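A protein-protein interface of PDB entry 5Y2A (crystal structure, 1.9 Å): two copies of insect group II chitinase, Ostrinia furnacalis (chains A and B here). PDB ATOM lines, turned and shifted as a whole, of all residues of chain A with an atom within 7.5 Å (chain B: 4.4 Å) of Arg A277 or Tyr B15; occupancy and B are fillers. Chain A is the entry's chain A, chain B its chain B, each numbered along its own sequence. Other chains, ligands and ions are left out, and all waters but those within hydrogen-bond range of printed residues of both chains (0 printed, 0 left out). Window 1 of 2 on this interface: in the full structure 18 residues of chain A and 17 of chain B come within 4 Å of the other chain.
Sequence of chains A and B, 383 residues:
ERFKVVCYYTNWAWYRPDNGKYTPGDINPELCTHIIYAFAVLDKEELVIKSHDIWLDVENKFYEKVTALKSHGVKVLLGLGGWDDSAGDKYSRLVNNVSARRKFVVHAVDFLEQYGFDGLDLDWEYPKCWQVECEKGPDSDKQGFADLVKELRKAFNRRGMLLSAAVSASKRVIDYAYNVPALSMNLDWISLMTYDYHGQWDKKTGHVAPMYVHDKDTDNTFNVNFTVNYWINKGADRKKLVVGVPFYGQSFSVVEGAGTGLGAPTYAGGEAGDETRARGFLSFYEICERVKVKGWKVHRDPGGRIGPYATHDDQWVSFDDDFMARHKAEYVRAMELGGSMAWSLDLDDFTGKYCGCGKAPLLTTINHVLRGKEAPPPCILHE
The backbone carbonyl oxygen (O) of Tyr A15 lies within hydrogen-bond range of the guanidinium group (NH2) of Arg A277 (2.5 Å).
The indole nitrogen (NE1) of Trp B12 sits close to a ring nitrogen (NE2) of His B52, 3.5 Å away.
The indole nitrogen of Trp B12 sits at hydrogen-bond distance from the side-chain carboxylate of Asp B53 (2.8 Å).
The side-chain carboxylate of Asp B53 lies within hydrogen-bond range of the side-chain hydroxyl of Tyr B15, 2.6 Å away.
The side-chain carboxylate of Asp B53 lies close to the backbone NH of Trp B55.
The side-chain carboxylate of Asp B53 lies within hydrogen-bond range of the backbone NH of Leu B56, 3.2 Å away.
The guanidinium group of Arg A277 sits at hydrogen-bond distance from the side-chain hydroxyl of Tyr B15 (3.1 Å).
The guanidinium group (NH1) of Arg A277 lies within salt-bridge range of the side-chain carboxylate (OD1) of Asp B53 (2.9 Å).
Among the printed residues, merely in contact across the chains: Trp A14 with Trp B55, Tyr A15 with Trp B14, Tyr A15 with Trp B55, Arg A16 with Trp B55, Pro A17 with Trp B55, Arg A277 with His B52 and Arg A277 with Trp B55.
Of the 21 printed residues of chain A, 5 touch a printed residue of chain B.
Printed residues of chain B that touch a printed residue of chain A: Trp B14, Tyr B15, His B52, Asp B53 and Trp B55.
Tyr A15 touches Trp B14, but with the chains exchanged Trp A14 does not touch Tyr B15 (8.2 Å).
Printed residues of chain B within 4 Å of Tyr A15: Trp B14 and Trp B55.
Of the printed residues of chain B, Arg A16 touches Trp B55 (3.2 Å).
Of chain B, only Tyr B15 (3.1 Å), His B52 (3.9 Å), Asp B53 (2.9 Å) and Trp B55 (3.8 Å) come within 4 Å of Arg A277.
Ala A278 touches none of the printed residues of chain B.
Glu A286 touches none of the printed residues of chain B.
Printed residues of chain A within 4 Å of Trp B14: Tyr A15 (3.6 Å).
The nearest printed residue of chain B that does not touch Arg A277 is Trp B12 (4.2 Å).
The nearest printed residue of chain B that does not touch Trp A14 is Trp B14 (6.1 Å).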
ATOM      1  N   TRP A  12      21.876 -14.265 -12.732  1.00  0.00           N
ATOM      2  CA  TRP A  12      20.771 -15.089 -13.227  1.00  0.00           C
ATOM      3  C   TRP A  12      20.587 -16.410 -12.471  1.00  0.00           C
ATOM      4  O   TRP A  12      19.593 -17.107 -12.712  1.00  0.00           O
ATOM      5  CB  TRP A  12      20.947 -15.354 -14.722  1.00  0.00           C
ATOM      6  CG  TRP A  12      22.125 -16.204 -15.095  1.00  0.00           C
ATOM      7  CD1 TRP A  12      22.155 -17.567 -15.211  1.00  0.00           C
ATOM      8  CD2 TRP A  12      23.448 -15.745 -15.406  1.00  0.00           C
ATOM      9  NE1 TRP A  12      23.414 -17.983 -15.585  1.00  0.00           N
ATOM     10  CE2 TRP A  12      24.228 -16.885 -15.708  1.00  0.00           C
ATOM     11  CE3 TRP A  12      24.050 -14.481 -15.458  1.00  0.00           C
ATOM     12  CZ2 TRP A  12      25.577 -16.799 -16.066  1.00  0.00           C
ATOM     13  CZ3 TRP A  12      25.394 -14.397 -15.803  1.00  0.00           C
ATOM     14  CH2 TRP A  12      26.141 -15.549 -16.107  1.00  0.00           C
ATOM     15  N   ALA A  13      21.483 -16.768 -11.548  1.00  0.00           N
ATOM     16  CA  ALA A  13      21.294 -17.978 -10.747  1.00  0.00           C
ATOM     17  C   ALA A  13      20.129 -17.868  -9.775  1.00  0.00           C
ATOM     18  O   ALA A  13      19.781 -18.867  -9.135  1.00  0.00           O
ATOM     19  CB  ALA A  13      22.573 -18.323  -9.981  1.00  0.00           C
ATOM     20  N   TRP A  14      19.595 -16.665  -9.573  1.00  0.00           N
ATOM     21  CA  TRP A  14      18.394 -16.495  -8.764  1.00  0.00           C
ATOM     22  C   TRP A  14      17.168 -17.102  -9.445  1.00  0.00           C
ATOM     23  O   TRP A  14      16.243 -17.562  -8.765  1.00  0.00           O
ATOM     24  CB  TRP A  14      18.192 -15.004  -8.489  1.00  0.00           C
ATOM     25  CG  TRP A  14      17.120 -14.689  -7.495  1.00  0.00           C
ATOM     26  CD1 TRP A  14      17.263 -14.579  -6.141  1.00  0.00           C
ATOM     27  CD2 TRP A  14      15.745 -14.412  -7.778  1.00  0.00           C
ATOM     28  NE1 TRP A  14      16.057 -14.265  -5.564  1.00  0.00           N
ATOM     29  CE2 TRP A  14      15.108 -14.156  -6.547  1.00  0.00           C
ATOM     30  CE3 TRP A  14      14.987 -14.365  -8.952  1.00  0.00           C
ATOM     31  CZ2 TRP A  14      13.749 -13.859  -6.457  1.00  0.00           C
ATOM     32  CZ3 TRP A  14      13.640 -14.068  -8.861  1.00  0.00           C
ATOM     33  CH2 TRP A  14      13.035 -13.819  -7.624  1.00  0.00           C
ATOM     34  N   TYR A  15      17.147 -17.112 -10.780  1.00  0.00           N
ATOM     35  CA  TYR A  15      15.995 -17.577 -11.559  1.00  0.00           C
ATOM     36  C   TYR A  15      16.080 -19.086 -11.786  1.00  0.00           C
ATOM     37  O   TYR A  15      16.088 -19.583 -12.908  1.00  0.00           O
ATOM     38  CB  TYR A  15      15.922 -16.832 -12.889  1.00  0.00           C
ATOM     39  CG  TYR A  15      15.827 -15.327 -12.769  1.00  0.00           C
ATOM     40  CD1 TYR A  15      14.651 -14.720 -12.366  1.00  0.00           C
ATOM     41  CD2 TYR A  15      16.900 -14.512 -13.103  1.00  0.00           C
ATOM     42  CE1 TYR A  15      14.545 -13.354 -12.261  1.00  0.00           C
ATOM     43  CE2 TYR A  15      16.802 -13.130 -13.007  1.00  0.00           C
ATOM     44  CZ  TYR A  15      15.616 -12.561 -12.580  1.00  0.00           C
ATOM     45  OH  TYR A  15      15.483 -11.200 -12.474  1.00  0.00           O
ATOM     46  N   ARG A  16      16.170 -19.814 -10.685  1.00  0.00           N
ATOM     47  CA  ARG A  16      16.441 -21.240 -10.708  1.00  0.00           C
ATOM     48  C   ARG A  16      15.554 -21.935  -9.693  1.00  0.00           C
ATOM     49  O   ARG A  16      15.232 -21.347  -8.653  1.00  0.00           O
ATOM     50  CB  ARG A  16      17.910 -21.524 -10.372  1.00  0.00           C
ATOM     51  CG  ARG A  16      18.622 -22.374 -11.377  1.00  0.00           C
ATOM     52  CD  ARG A  16      20.118 -22.280 -11.197  1.00  0.00           C
ATOM     53  NE  ARG A  16      20.726 -21.559 -12.305  1.00  0.00           N
ATOM     54  CZ  ARG A  16      22.028 -21.348 -12.430  1.00  0.00           C
ATOM     55  NH1 ARG A  16      22.863 -21.817 -11.513  1.00  0.00           N
ATOM     56  NH2 ARG A  16      22.494 -20.674 -13.472  1.00  0.00           N
ATOM     57  N   PRO A  17      15.181 -23.198  -9.938  1.00  0.00           N
ATOM     58  CA  PRO A  17      14.326 -23.896  -8.972  1.00  0.00           C
ATOM     59  C   PRO A  17      15.029 -23.924  -7.623  1.00  0.00           C
ATOM     60  O   PRO A  17      16.260 -23.930  -7.547  1.00  0.00           O
ATOM     61  CB  PRO A  17      14.181 -25.303  -9.569  1.00  0.00           C
ATOM     62  CG  PRO A  17      14.419 -25.115 -11.043  1.00  0.00           C
ATOM     63  CD  PRO A  17      15.408 -23.990 -11.163  1.00  0.00           C
ATOM     64  N   HIS A  52      22.011  -5.420 -16.568  1.00  0.00           N
ATOM     65  CA  HIS A  52      21.260  -6.334 -17.413  1.00  0.00           C
ATOM     66  C   HIS A  52      19.965  -6.777 -16.752  1.00  0.00           C
ATOM     67  O   HIS A  52      19.104  -7.355 -17.424  1.00  0.00           O
ATOM     68  CB  HIS A  52      22.127  -7.559 -17.757  1.00  0.00           C
ATOM     69  CG  HIS A  52      21.464  -8.538 -18.679  1.00  0.00           C
ATOM     70  ND1 HIS A  52      20.915  -9.724 -18.239  1.00  0.00           N
ATOM     71  CD2 HIS A  52      21.247  -8.497 -20.016  1.00  0.00           C
ATOM     72  CE1 HIS A  52      20.395 -10.375 -19.266  1.00  0.00           C
ATOM     73  NE2 HIS A  52      20.583  -9.651 -20.355  1.00  0.00           N
ATOM     74  N   ASP A  84      26.702 -13.956 -24.193  1.00  0.00           N
ATOM     75  CA  ASP A  84      25.454 -13.484 -24.790  1.00  0.00           C
ATOM     76  C   ASP A  84      25.534 -12.010 -25.168  1.00  0.00           C
ATOM     77  O   ASP A  84      25.039 -11.608 -26.229  1.00  0.00           O
ATOM     78  CB  ASP A  84      24.287 -13.715 -23.827  1.00  0.00           C
ATOM     79  CG  ASP A  84      22.978 -13.135 -24.345  1.00  0.00           C
ATOM     80  OD1 ASP A  84      22.748 -13.185 -25.572  1.00  0.00           O
ATOM     81  OD2 ASP A  84      22.181 -12.623 -23.531  1.00  0.00           O
ATOM     82  N   GLU A 271      20.377 -34.193 -22.388  1.00  0.00           N
ATOM     83  CA  GLU A 271      19.149 -33.786 -21.708  1.00  0.00           C
ATOM     84  C   GLU A 271      19.447 -32.722 -20.659  1.00  0.00           C
ATOM     85  O   GLU A 271      20.460 -32.787 -19.957  1.00  0.00           O
ATOM     86  CB  GLU A 271      18.496 -34.996 -21.025  1.00  0.00           C
ATOM     87  CG  GLU A 271      17.919 -36.067 -21.942  1.00  0.00           C
ATOM     88  CD  GLU A 271      16.654 -35.602 -22.652  1.00  0.00           C
ATOM     89  OE1 GLU A 271      15.811 -34.961 -21.992  1.00  0.00           O
ATOM     90  OE2 GLU A 271      16.502 -35.874 -23.856  1.00  0.00           O
ATOM     91  N   ALA A 272      18.557 -31.737 -20.556  1.00  0.00           N
ATOM     92  CA  ALA A 272      18.762 -30.639 -19.618  1.00  0.00           C
ATOM     93  C   ALA A 272      18.638 -31.121 -18.177  1.00  0.00           C
ATOM     94  O   ALA A 272      17.875 -32.037 -17.870  1.00  0.00           O
ATOM     95  CB  ALA A 272      17.750 -29.523 -19.870  1.00  0.00           C
ATOM     96  N   GLY A 273      19.400 -30.482 -17.282  1.00  0.00           N
ATOM     97  CA  GLY A 273      19.241 -30.740 -15.868  1.00  0.00           C
ATOM     98  C   GLY A 273      18.021 -30.045 -15.284  1.00  0.00           C
ATOM     99  O   GLY A 273      17.525 -29.050 -15.821  1.00  0.00           O
ATOM    100  N   ASP A 274      17.553 -30.566 -14.141  1.00  0.00           N
ATOM    101  CA  ASP A 274      16.354 -30.018 -13.505  1.00  0.00           C
ATOM    102  C   ASP A 274      16.562 -28.574 -13.074  1.00  0.00           C
ATOM    103  O   ASP A 274      15.630 -27.760 -13.110  1.00  0.00           O
ATOM    104  CB  ASP A 274      15.958 -30.843 -12.279  1.00  0.00           C
ATOM    105  CG  ASP A 274      15.522 -32.251 -12.622  1.00  0.00           C
ATOM    106  OD1 ASP A 274      15.326 -32.559 -13.817  1.00  0.00           O
ATOM    107  OD2 ASP A 274      15.355 -33.045 -11.673  1.00  0.00           O
ATOM    108  N   GLU A 275      17.768 -28.243 -12.635  1.00  0.00           N
ATOM    109  CA  GLU A 275      18.009 -26.907 -12.109  1.00  0.00           C
ATOM    110  C   GLU A 275      18.569 -25.958 -13.156  1.00  0.00           C
ATOM    111  O   GLU A 275      18.137 -24.803 -13.230  1.00  0.00           O
ATOM    112  CB  GLU A 275      18.966 -26.979 -10.915  1.00  0.00           C
ATOM    113  CG  GLU A 275      18.311 -27.467  -9.633  1.00  0.00           C
ATOM    114  CD  GLU A 275      18.198 -28.978  -9.561  1.00  0.00           C
ATOM    115  OE1 GLU A 275      19.098 -29.685 -10.061  1.00  0.00           O
ATOM    116  OE2 GLU A 275      17.192 -29.459  -9.001  1.00  0.00           O
ATOM    117  N   THR A 276      19.512 -26.410 -13.983  1.00  0.00           N
ATOM    118  CA  THR A 276      20.119 -25.493 -14.940  1.00  0.00           C
ATOM    119  C   THR A 276      19.336 -25.368 -16.243  1.00  0.00           C
ATOM    120  O   THR A 276      19.461 -24.341 -16.920  1.00  0.00           O
ATOM    121  CB  THR A 276      21.579 -25.898 -15.221  1.00  0.00           C
ATOM    122  OG1 THR A 276      21.658 -27.271 -15.631  1.00  0.00           O
ATOM    123  CG2 THR A 276      22.431 -25.681 -13.956  1.00  0.00           C
ATOM    124  N   ARG A 277      18.525 -26.363 -16.596  1.00  0.00           N
ATOM    125  CA  ARG A 277      17.540 -26.247 -17.679  1.00  0.00           C
ATOM    126  C   ARG A 277      18.167 -25.760 -18.983  1.00  0.00           C
ATOM    127  O   ARG A 277      17.636 -24.884 -19.666  1.00  0.00           O
ATOM    128  CB  ARG A 277      16.405 -25.313 -17.252  1.00  0.00           C
ATOM    129  CG  ARG A 277      15.738 -25.711 -15.952  1.00  0.00           C
ATOM    130  CD  ARG A 277      14.995 -24.527 -15.355  1.00  0.00           C
ATOM    131  NE  ARG A 277      16.020 -23.624 -14.835  1.00  0.00           N
ATOM    132  CZ  ARG A 277      15.871 -22.324 -14.605  1.00  0.00           C
ATOM    133  NH1 ARG A 277      14.712 -21.716 -14.827  1.00  0.00           N
ATOM    134  NH2 ARG A 277      16.907 -21.631 -14.159  1.00  0.00           N
ATOM    135  N   ALA A 278      19.301 -26.349 -19.348  1.00  0.00           N
ATOM    136  CA  ALA A 278      19.960 -25.956 -20.591  1.00  0.00           C
ATOM    137  C   ALA A 278      20.610 -27.189 -21.194  1.00  0.00           C
ATOM    138  O   ALA A 278      21.616 -27.672 -20.667  1.00  0.00           O
ATOM    139  CB  ALA A 278      20.991 -24.854 -20.338  1.00  0.00           C
ATOM    140  N   ARG A 279      20.075 -27.664 -22.319  1.00  0.00           N
ATOM    141  CA  ARG A 279      20.661 -28.832 -22.958  1.00  0.00           C
ATOM    142  C   ARG A 279      22.116 -28.542 -23.317  1.00  0.00           C
ATOM    143  O   ARG A 279      22.456 -27.447 -23.768  1.00  0.00           O
ATOM    144  CB  ARG A 279      19.875 -29.208 -24.217  1.00  0.00           C
ATOM    145  CG  ARG A 279      18.431 -29.707 -23.992  1.00  0.00           C
ATOM    146  CD  ARG A 279      17.850 -30.135 -25.337  1.00  0.00           C
ATOM    147  NE  ARG A 279      18.566 -31.305 -25.845  1.00  0.00           N
ATOM    148  CZ  ARG A 279      18.153 -32.562 -25.715  1.00  0.00           C
ATOM    149  NH1 ARG A 279      16.978 -32.827 -25.158  1.00  0.00           N
ATOM    150  NH2 ARG A 279      18.894 -33.553 -26.188  1.00  0.00           N
ATOM    151  N   GLY A 280      22.975 -29.537 -23.122  1.00  0.00           N
ATOM    152  CA  GLY A 280      24.403 -29.387 -23.335  1.00  0.00           C
ATOM    153  C   GLY A 280      25.193 -28.991 -22.107  1.00  0.00           C
ATOM    154  O   GLY A 280      26.426 -28.965 -22.172  1.00  0.00           O
ATOM    155  N   PHE A 281      24.528 -28.782 -20.972  1.00  0.00           N
ATOM    156  CA  PHE A 281      25.129 -28.176 -19.796  1.00  0.00           C
ATOM    157  C   PHE A 281      24.572 -28.872 -18.560  1.00  0.00           C
ATOM    158  O   PHE A 281      23.370 -29.136 -18.486  1.00  0.00           O
ATOM    159  CB  PHE A 281      24.815 -26.664 -19.789  1.00  0.00           C
ATOM    160  CG  PHE A 281      25.336 -25.921 -18.599  1.00  0.00           C
ATOM    161  CD1 PHE A 281      24.617 -25.879 -17.411  1.00  0.00           C
ATOM    162  CD2 PHE A 281      26.521 -25.208 -18.685  1.00  0.00           C
ATOM    163  CE1 PHE A 281      25.091 -25.175 -16.321  1.00  0.00           C
ATOM    164  CE2 PHE A 281      27.001 -24.497 -17.594  1.00  0.00           C
ATOM    165  CZ  PHE A 281      26.283 -24.481 -16.414  1.00  0.00           C
ATOM    166  N   LEU A 282      25.447 -29.196 -17.607  1.00  0.00           N
ATOM    167  CA  LEU A 282      25.026 -29.725 -16.310  1.00  0.00           C
ATOM    168  C   LEU A 282      25.936 -29.152 -15.236  1.00  0.00           C
ATOM    169  O   LEU A 282      27.160 -29.153 -15.401  1.00  0.00           O
ATOM    170  CB  LEU A 282      25.085 -31.263 -16.267  1.00  0.00           C
ATOM    171  CG  LEU A 282      24.124 -32.075 -17.146  1.00  0.00           C
ATOM    172  CD1 LEU A 282      24.491 -33.561 -17.119  1.00  0.00           C
ATOM    173  CD2 LEU A 282      22.675 -31.876 -16.700  1.00  0.00           C
ATOM    174  N   GLU A 286      24.362 -31.314 -10.365  1.00  0.00           N
ATOM    175  CA  GLU A 286      23.502 -32.168 -11.184  1.00  0.00           C
ATOM    176  C   GLU A 286      24.241 -33.431 -11.619  1.00  0.00           C
ATOM    177  O   GLU A 286      23.640 -34.504 -11.748  1.00  0.00           O
ATOM    178  CB  GLU A 286      22.992 -31.388 -12.401  1.00  0.00           C
ATOM    179  CG  GLU A 286      21.959 -30.322 -12.046  1.00  0.00           C
ATOM    180  CD  GLU A 286      21.614 -29.399 -13.210  1.00  0.00           C
ATOM    181  OE1 GLU A 286      22.517 -29.032 -13.996  1.00  0.00           O
ATOM    182  OE2 GLU A 286      20.429 -29.020 -13.326  1.00  0.00           O
ATOM    183  N   TRP B  12       9.570 -19.628 -22.506  1.00  0.00           N
ATOM    184  CA  TRP B  12      10.894 -19.040 -22.336  1.00  0.00           C
ATOM    185  C   TRP B  12      11.032 -17.752 -23.141  1.00  0.00           C
ATOM    186  O   TRP B  12      12.138 -17.254 -23.348  1.00  0.00           O
ATOM    187  CB  TRP B  12      11.980 -20.036 -22.748  1.00  0.00           C
ATOM    188  CG  TRP B  12      12.166 -21.158 -21.772  1.00  0.00           C
ATOM    189  CD1 TRP B  12      11.726 -21.203 -20.482  1.00  0.00           C
ATOM    190  CD2 TRP B  12      12.844 -22.398 -22.009  1.00  0.00           C
ATOM    191  NE1 TRP B  12      12.086 -22.393 -19.900  1.00  0.00           N
ATOM    192  CE2 TRP B  12      12.774 -23.145 -20.816  1.00  0.00           C
ATOM    193  CE3 TRP B  12      13.501 -22.948 -23.112  1.00  0.00           C
ATOM    194  CZ2 TRP B  12      13.337 -24.414 -20.696  1.00  0.00           C
ATOM    195  CZ3 TRP B  12      14.060 -24.208 -22.991  1.00  0.00           C
ATOM    196  CH2 TRP B  12      13.974 -24.927 -21.792  1.00  0.00           C
ATOM    197  N   ALA B  13       9.898 -17.185 -23.539  1.00  0.00           N
ATOM    198  CA  ALA B  13       9.864 -15.782 -23.934  1.00  0.00           C
ATOM    199  C   ALA B  13       9.974 -14.884 -22.689  1.00  0.00           C
ATOM    200  O   ALA B  13      10.279 -13.753 -22.781  1.00  0.00           O
ATOM    201  CB  ALA B  13       8.655 -15.458 -24.766  1.00  0.00           C
ATOM    202  N   TRP B  14       9.737 -15.464 -21.527  1.00  0.00           N
ATOM    203  CA  TRP B  14       9.847 -14.682 -20.294  1.00  0.00           C
ATOM    204  C   TRP B  14      11.262 -14.144 -20.090  1.00  0.00           C
ATOM    205  O   TRP B  14      11.445 -13.100 -19.465  1.00  0.00           O
ATOM    206  CB  TRP B  14       9.430 -15.549 -19.093  1.00  0.00           C
ATOM    207  CG  TRP B  14       9.303 -14.764 -17.812  1.00  0.00           C
ATOM    208  CD1 TRP B  14       8.188 -14.133 -17.344  1.00  0.00           C
ATOM    209  CD2 TRP B  14      10.336 -14.529 -16.839  1.00  0.00           C
ATOM    210  NE1 TRP B  14       8.461 -13.517 -16.143  1.00  0.00           N
ATOM    211  CE2 TRP B  14       9.771 -13.741 -15.814  1.00  0.00           C
ATOM    212  CE3 TRP B  14      11.677 -14.907 -16.736  1.00  0.00           C
ATOM    213  CZ2 TRP B  14      10.502 -13.327 -14.697  1.00  0.00           C
ATOM    214  CZ3 TRP B  14      12.404 -14.491 -15.630  1.00  0.00           C
ATOM    215  CH2 TRP B  14      11.812 -13.711 -14.624  1.00  0.00           C
ATOM    216  N   TYR B  15      12.270 -14.844 -20.614  1.00  0.00           N
ATOM    217  CA  TYR B  15      13.662 -14.465 -20.391  1.00  0.00           C
ATOM    218  C   TYR B  15      14.173 -13.423 -21.380  1.00  0.00           C
ATOM    219  O   TYR B  15      15.330 -13.014 -21.276  1.00  0.00           O
ATOM    220  CB  TYR B  15      14.554 -15.715 -20.440  1.00  0.00           C
ATOM    221  CG  TYR B  15      14.212 -16.755 -19.380  1.00  0.00           C
ATOM    222  CD1 TYR B  15      14.612 -16.581 -18.058  1.00  0.00           C
ATOM    223  CD2 TYR B  15      13.473 -17.887 -19.697  1.00  0.00           C
ATOM    224  CE1 TYR B  15      14.306 -17.526 -17.080  1.00  0.00           C
ATOM    225  CE2 TYR B  15      13.153 -18.837 -18.723  1.00  0.00           C
ATOM    226  CZ  TYR B  15      13.574 -18.644 -17.420  1.00  0.00           C
ATOM    227  OH  TYR B  15      13.269 -19.571 -16.447  1.00  0.00           O
ATOM    228  N   ARG B  16      13.337 -12.956 -22.312  1.00  0.00           N
ATOM    229  CA  ARG B  16      13.846 -12.031 -23.313  1.00  0.00           C
ATOM    230  C   ARG B  16      13.974 -10.626 -22.721  1.00  0.00           C
ATOM    231  O   ARG B  16      13.185 -10.235 -21.855  1.00  0.00           O
ATOM    232  CB  ARG B  16      12.922 -12.001 -24.531  1.00  0.00           C
ATOM    233  CG  ARG B  16      12.900 -13.312 -25.278  1.00  0.00           C
ATOM    234  CD  ARG B  16      12.225 -13.217 -26.636  1.00  0.00           C
ATOM    235  NE  ARG B  16      12.283 -14.516 -27.295  1.00  0.00           N
ATOM    236  CZ  ARG B  16      11.250 -15.120 -27.869  1.00  0.00           C
ATOM    237  NH1 ARG B  16      10.058 -14.537 -27.893  1.00  0.00           N
ATOM    238  NH2 ARG B  16      11.416 -16.316 -28.419  1.00  0.00           N
ATOM    239  N   PRO B  17      14.982  -9.868 -23.151  1.00  0.00           N
ATOM    240  CA  PRO B  17      15.196  -8.526 -22.599  1.00  0.00           C
ATOM    241  C   PRO B  17      14.180  -7.487 -23.051  1.00  0.00           C
ATOM    242  O   PRO B  17      13.606  -7.563 -24.142  1.00  0.00           O
ATOM    243  CB  PRO B  17      16.600  -8.164 -23.102  1.00  0.00           C
ATOM    244  CG  PRO B  17      16.712  -8.888 -24.391  1.00  0.00           C
ATOM    245  CD  PRO B  17      15.970 -10.197 -24.195  1.00  0.00           C
ATOM    246  N   HIS B  52       9.627 -28.484 -18.327  1.00  0.00           N
ATOM    247  CA  HIS B  52      10.921 -28.147 -18.836  1.00  0.00           C
ATOM    248  C   HIS B  52      11.555 -27.009 -18.043  1.00  0.00           C
ATOM    249  O   HIS B  52      12.690 -26.731 -18.206  1.00  0.00           O
ATOM    250  CB  HIS B  52      10.905 -27.793 -20.329  1.00  0.00           C
ATOM    251  CG  HIS B  52      10.398 -26.419 -20.635  1.00  0.00           C
ATOM    252  ND1 HIS B  52      10.723 -25.732 -21.783  1.00  0.00           N
ATOM    253  CD2 HIS B  52       9.572 -25.609 -19.948  1.00  0.00           C
ATOM    254  CE1 HIS B  52      10.133 -24.557 -21.778  1.00  0.00           C
ATOM    255  NE2 HIS B  52       9.413 -24.463 -20.683  1.00  0.00           N
ATOM    256  N   ASP B  53      10.796 -26.356 -17.197  1.00  0.00           N
ATOM    257  CA  ASP B  53      11.271 -25.196 -16.426  1.00  0.00           C
ATOM    258  C   ASP B  53      10.473 -25.190 -15.122  1.00  0.00           C
ATOM    259  O   ASP B  53       9.427 -24.544 -15.022  1.00  0.00           O
ATOM    260  CB  ASP B  53      11.106 -23.894 -17.194  1.00  0.00           C
ATOM    261  CG  ASP B  53      11.801 -22.710 -16.515  1.00  0.00           C
ATOM    262  OD1 ASP B  53      12.086 -22.772 -15.298  1.00  0.00           O
ATOM    263  OD2 ASP B  53      12.058 -21.709 -17.210  1.00  0.00           O
ATOM    264  N   TRP B  55      11.074 -23.810 -12.358  1.00  0.00           N
ATOM    265  CA  TRP B  55      11.022 -22.511 -11.693  1.00  0.00           C
ATOM    266  C   TRP B  55       9.888 -21.641 -12.233  1.00  0.00           C
ATOM    267  O   TRP B  55       9.122 -21.047 -11.463  1.00  0.00           O
ATOM    268  CB  TRP B  55      12.371 -21.801 -11.831  1.00  0.00           C
ATOM    269  CG  TRP B  55      12.365 -20.483 -11.133  1.00  0.00           C
ATOM    270  CD1 TRP B  55      12.466 -20.260  -9.791  1.00  0.00           C
ATOM    271  CD2 TRP B  55      12.223 -19.207 -11.747  1.00  0.00           C
ATOM    272  NE1 TRP B  55      12.398 -18.912  -9.531  1.00  0.00           N
ATOM    273  CE2 TRP B  55      12.251 -18.243 -10.719  1.00  0.00           C
ATOM    274  CE3 TRP B  55      12.084 -18.780 -13.070  1.00  0.00           C
ATOM    275  CZ2 TRP B  55      12.138 -16.884 -10.973  1.00  0.00           C
ATOM    276  CZ3 TRP B  55      11.974 -17.423 -13.318  1.00  0.00           C
ATOM    277  CH2 TRP B  55      11.993 -16.497 -12.276  1.00  0.00           C
ATOM    278  N   LEU B  56       9.749 -21.565 -13.555  1.00  0.00           N
ATOM    279  CA  LEU B  56       8.657 -20.794 -14.138  1.00  0.00           C
ATOM    280  C   LEU B  56       7.334 -21.555 -14.075  1.00  0.00           C
ATOM    281  O   LEU B  56       6.326 -21.022 -13.593  1.00  0.00           O
ATOM    282  CB  LEU B  56       8.987 -20.447 -15.585  1.00  0.00           C
ATOM    283  CG  LEU B  56       9.684 -19.145 -15.974  1.00  0.00           C
ATOM    284  CD1 LEU B  56       9.521 -18.978 -17.465  1.00  0.00           C
ATOM    285  CD2 LEU B  56       9.116 -17.944 -15.243  1.00  0.00           C
